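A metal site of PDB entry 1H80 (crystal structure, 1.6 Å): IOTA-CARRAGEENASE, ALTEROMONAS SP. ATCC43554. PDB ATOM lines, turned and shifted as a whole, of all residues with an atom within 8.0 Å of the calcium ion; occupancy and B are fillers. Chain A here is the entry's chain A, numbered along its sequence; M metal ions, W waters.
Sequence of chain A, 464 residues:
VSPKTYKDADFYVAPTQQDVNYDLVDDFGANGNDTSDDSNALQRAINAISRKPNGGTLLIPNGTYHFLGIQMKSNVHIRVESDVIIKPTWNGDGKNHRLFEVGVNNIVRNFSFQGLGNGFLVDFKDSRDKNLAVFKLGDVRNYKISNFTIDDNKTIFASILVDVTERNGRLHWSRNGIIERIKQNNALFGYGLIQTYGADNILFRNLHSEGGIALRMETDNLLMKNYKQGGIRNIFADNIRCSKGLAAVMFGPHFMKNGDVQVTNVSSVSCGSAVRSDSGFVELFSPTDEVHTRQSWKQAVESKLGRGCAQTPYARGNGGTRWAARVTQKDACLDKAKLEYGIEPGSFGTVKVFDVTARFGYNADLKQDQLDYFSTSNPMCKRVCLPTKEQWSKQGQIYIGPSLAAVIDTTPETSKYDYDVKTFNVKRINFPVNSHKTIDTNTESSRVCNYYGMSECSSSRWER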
ATOM      1  N   ASN A  62       5.894 -18.182 -23.054  1.00  0.00           N
ATOM      2  CA  ASN A  62       6.696 -18.611 -21.919  1.00  0.00           C
ATOM      3  C   ASN A  62       8.103 -18.025 -21.941  1.00  0.00           C
ATOM      4  O   ASN A  62       8.778 -18.016 -22.972  1.00  0.00           O
ATOM      5  CB  ASN A  62       6.750 -20.126 -21.851  1.00  0.00           C
ATOM      6  CG  ASN A  62       5.438 -20.721 -21.408  1.00  0.00           C
ATOM      7  OD1 ASN A  62       4.747 -20.138 -20.579  1.00  0.00           O
ATOM      8  ND2 ASN A  62       5.096 -21.890 -21.935  1.00  0.00           N
ATOM      9  N   VAL A  80      -1.317 -14.333 -21.554  1.00  0.00           N
ATOM     10  CA  VAL A  80      -0.007 -14.741 -21.076  1.00  0.00           C
ATOM     11  C   VAL A  80       0.105 -16.237 -20.846  1.00  0.00           C
ATOM     12  O   VAL A  80      -0.713 -16.825 -20.155  1.00  0.00           O
ATOM     13  CB  VAL A  80       0.302 -14.009 -19.754  1.00  0.00           C
ATOM     14  CG1 VAL A  80       1.741 -14.247 -19.354  1.00  0.00           C
ATOM     15  CG2 VAL A  80       0.010 -12.520 -19.906  1.00  0.00           C
ATOM     16  N   GLU A  81       1.133 -16.862 -21.424  1.00  0.00           N
ATOM     17  CA  GLU A  81       1.280 -18.294 -21.230  1.00  0.00           C
ATOM     18  C   GLU A  81       1.537 -18.631 -19.768  1.00  0.00           C
ATOM     19  O   GLU A  81       2.057 -17.806 -19.005  1.00  0.00           O
ATOM     20  CB  GLU A  81       2.360 -18.866 -22.149  1.00  0.00           C
ATOM     21  CG  GLU A  81       1.934 -18.784 -23.621  1.00  0.00           C
ATOM     22  CD  GLU A  81       2.741 -19.685 -24.533  1.00  0.00           C
ATOM     23  OE1 GLU A  81       3.994 -19.659 -24.451  1.00  0.00           O
ATOM     24  OE2 GLU A  81       2.130 -20.422 -25.341  1.00  0.00           O
ATOM     25  N   SER A  82       1.185 -19.851 -19.386  1.00  0.00           N
ATOM     26  CA  SER A  82       1.250 -20.303 -18.003  1.00  0.00           C
ATOM     27  C   SER A  82       2.578 -20.396 -17.265  1.00  0.00           C
ATOM     28  O   SER A  82       2.595 -20.444 -16.033  1.00  0.00           O
ATOM     29  CB  SER A  82       0.520 -21.631 -17.883  1.00  0.00           C
ATOM     30  OG  SER A  82       0.321 -21.989 -16.527  1.00  0.00           O
ATOM     31  N   ASP A  83       3.697 -20.442 -17.994  1.00  0.00           N
ATOM     32  CA  ASP A  83       4.996 -20.523 -17.329  1.00  0.00           C
ATOM     33  C   ASP A  83       5.736 -19.197 -17.378  1.00  0.00           C
ATOM     34  O   ASP A  83       6.913 -19.112 -17.038  1.00  0.00           O
ATOM     35  CB  ASP A  83       5.843 -21.625 -17.960  1.00  0.00           C
ATOM     36  CG  ASP A  83       5.263 -23.010 -17.752  1.00  0.00           C
ATOM     37  OD1 ASP A  83       4.900 -23.324 -16.598  1.00  0.00           O
ATOM     38  OD2 ASP A  83       5.170 -23.775 -18.730  1.00  0.00           O
ATOM     39  N   VAL A  84       5.028 -18.155 -17.798  1.00  0.00           N
ATOM     40  CA  VAL A  84       5.630 -16.831 -17.883  1.00  0.00           C
ATOM     41  C   VAL A  84       5.924 -16.248 -16.513  1.00  0.00           C
ATOM     42  O   VAL A  84       5.177 -16.452 -15.566  1.00  0.00           O
ATOM     43  CB  VAL A  84       4.710 -15.852 -18.645  1.00  0.00           C
ATOM     44  CG1 VAL A  84       5.210 -14.406 -18.463  1.00  0.00           C
ATOM     45  CG2 VAL A  84       4.696 -16.209 -20.117  1.00  0.00           C
ATOM     46  N   LEU A 116      -3.275 -17.538 -19.264  1.00  0.00           N
ATOM     47  CA  LEU A 116      -3.830 -18.766 -19.795  1.00  0.00           C
ATOM     48  C   LEU A 116      -3.617 -19.868 -18.761  1.00  0.00           C
ATOM     49  O   LEU A 116      -2.767 -19.746 -17.877  1.00  0.00           O
ATOM     50  CB  LEU A 116      -3.115 -19.155 -21.091  1.00  0.00           C
ATOM     51  CG  LEU A 116      -3.339 -18.225 -22.277  1.00  0.00           C
ATOM     52  CD1 LEU A 116      -2.288 -18.475 -23.335  1.00  0.00           C
ATOM     53  CD2 LEU A 116      -4.737 -18.441 -22.827  1.00  0.00           C
ATOM     54  N   GLY A 117      -4.394 -20.936 -18.873  1.00  0.00           N
ATOM     55  CA  GLY A 117      -4.233 -22.064 -17.965  1.00  0.00           C
ATOM     56  C   GLY A 117      -4.357 -21.724 -16.486  1.00  0.00           C
ATOM     57  O   GLY A 117      -5.298 -21.044 -16.091  1.00  0.00           O
ATOM     58  N   ASN A 118      -3.415 -22.210 -15.685  1.00  0.00           N
ATOM     59  CA  ASN A 118      -3.462 -21.950 -14.253  1.00  0.00           C
ATOM     60  C   ASN A 118      -2.821 -20.624 -13.857  1.00  0.00           C
ATOM     61  O   ASN A 118      -2.579 -20.362 -12.679  1.00  0.00           O
ATOM     62  CB  ASN A 118      -2.839 -23.102 -13.448  1.00  0.00           C
ATOM     63  CG  ASN A 118      -1.373 -23.335 -13.788  1.00  0.00           C
ATOM     64  OD1 ASN A 118      -0.669 -22.414 -14.176  1.00  0.00           O
ATOM     65  ND2 ASN A 118      -0.921 -24.574 -13.616  1.00  0.00           N
ATOM     66  N   GLY A 119      -2.541 -19.782 -14.839  1.00  0.00           N
ATOM     67  CA  GLY A 119      -1.975 -18.478 -14.549  1.00  0.00           C
ATOM     68  C   GLY A 119      -0.475 -18.385 -14.575  1.00  0.00           C
ATOM     69  O   GLY A 119       0.218 -19.390 -14.610  1.00  0.00           O
ATOM     70  N   PHE A 120       0.023 -17.156 -14.549  1.00  0.00           N
ATOM     71  CA  PHE A 120       1.461 -16.928 -14.588  1.00  0.00           C
ATOM     72  C   PHE A 120       1.925 -16.255 -13.311  1.00  0.00           C
ATOM     73  O   PHE A 120       1.147 -16.051 -12.380  1.00  0.00           O
ATOM     74  CB  PHE A 120       1.843 -16.064 -15.787  1.00  0.00           C
ATOM     75  CG  PHE A 120       1.164 -14.724 -15.819  1.00  0.00           C
ATOM     76  CD1 PHE A 120      -0.145 -14.604 -16.282  1.00  0.00           C
ATOM     77  CD2 PHE A 120       1.833 -13.591 -15.382  1.00  0.00           C
ATOM     78  CE1 PHE A 120      -0.770 -13.368 -16.313  1.00  0.00           C
ATOM     79  CE2 PHE A 120       1.212 -12.348 -15.405  1.00  0.00           C
ATOM     80  CZ  PHE A 120      -0.091 -12.237 -15.878  1.00  0.00           C
ATOM     81  N   LEU A 121       3.193 -15.901 -13.291  1.00  0.00           N
ATOM     82  CA  LEU A 121       3.767 -15.286 -12.112  1.00  0.00           C
ATOM     83  C   LEU A 121       4.337 -13.891 -12.324  1.00  0.00           C
ATOM     84  O   LEU A 121       5.017 -13.638 -13.317  1.00  0.00           O
ATOM     85  CB  LEU A 121       4.891 -16.191 -11.577  1.00  0.00           C
ATOM     86  CG  LEU A 121       5.648 -15.682 -10.350  1.00  0.00           C
ATOM     87  CD1 LEU A 121       4.755 -15.778  -9.131  1.00  0.00           C
ATOM     88  CD2 LEU A 121       6.907 -16.506 -10.148  1.00  0.00           C
ATOM     89  N   ASN A 147      -6.261 -13.978 -13.653  1.00  0.00           N
ATOM     90  CA  ASN A 147      -5.372 -15.120 -13.572  1.00  0.00           C
ATOM     91  C   ASN A 147      -3.850 -15.081 -13.481  1.00  0.00           C
ATOM     92  O   ASN A 147      -3.140 -15.438 -14.437  1.00  0.00           O
ATOM     93  CB  ASN A 147      -5.752 -16.018 -14.729  1.00  0.00           C
ATOM     94  CG  ASN A 147      -5.438 -17.474 -14.486  1.00  0.00           C
ATOM     95  OD1 ASN A 147      -5.321 -17.915 -13.343  1.00  0.00           O
ATOM     96  ND2 ASN A 147      -5.351 -18.237 -15.578  1.00  0.00           N
ATOM     97  N   PHE A 148      -3.335 -14.692 -12.319  1.00  0.00           N
ATOM     98  CA  PHE A 148      -1.902 -14.700 -12.097  1.00  0.00           C
ATOM     99  C   PHE A 148      -1.631 -14.615 -10.612  1.00  0.00           C
ATOM    100  O   PHE A 148      -2.512 -14.320  -9.811  1.00  0.00           O
ATOM    101  CB  PHE A 148      -1.216 -13.575 -12.881  1.00  0.00           C
ATOM    102  CG  PHE A 148      -1.766 -12.209 -12.618  1.00  0.00           C
ATOM    103  CD1 PHE A 148      -1.235 -11.420 -11.602  1.00  0.00           C
ATOM    104  CD2 PHE A 148      -2.781 -11.679 -13.412  1.00  0.00           C
ATOM    105  CE1 PHE A 148      -1.704 -10.126 -11.379  1.00  0.00           C
ATOM    106  CE2 PHE A 148      -3.254 -10.384 -13.202  1.00  0.00           C
ATOM    107  CZ  PHE A 148      -2.713  -9.605 -12.182  1.00  0.00           C
ATOM    108  N   THR A 149      -0.394 -14.945 -10.264  1.00  0.00           N
ATOM    109  CA  THR A 149       0.044 -14.929  -8.893  1.00  0.00           C
ATOM    110  C   THR A 149       1.098 -13.835  -8.788  1.00  0.00           C
ATOM    111  O   THR A 149       1.884 -13.630  -9.709  1.00  0.00           O
ATOM    112  CB  THR A 149       0.675 -16.272  -8.496  1.00  0.00           C
ATOM    113  OG1 THR A 149      -0.313 -17.300  -8.564  1.00  0.00           O
ATOM    114  CG2 THR A 149       1.249 -16.210  -7.086  1.00  0.00           C
HETATM  115 CA    CA M   1       1.338 -21.389 -14.317  1.00  0.00          CA
HETATM  116  O   HOH W   1       0.395 -20.743 -12.046  1.00  0.00           O
HETATM  117  O   HOH W   2       1.921 -22.867 -12.293  1.00  0.00           O
HETATM  118  O   HOH W   3       2.688 -23.172 -14.977  1.00  0.00           O
HETATM  119  O   HOH W   4       3.090 -20.129 -13.183  1.00  0.00           O
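N of Gly 119 sits close to ND2 of Asn 147, at 3.3 Å.
The nearest printed residue that does not touch the calcium ion is Phe 120 (4.4 Å).
The calcium ion is bound by OD1 of Asn 118 (2.3 Å), O of Gly 119 (2.3 Å), O of Ser 82 (2.3 Å), water W3 (2.3 Å), water W4 (2.4 Å), OG of Ser 82 (2.5 Å), water W1 (2.5 Å) and water W2 (2.6 Å). The calcium ion has eight donor atoms within binding distance.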
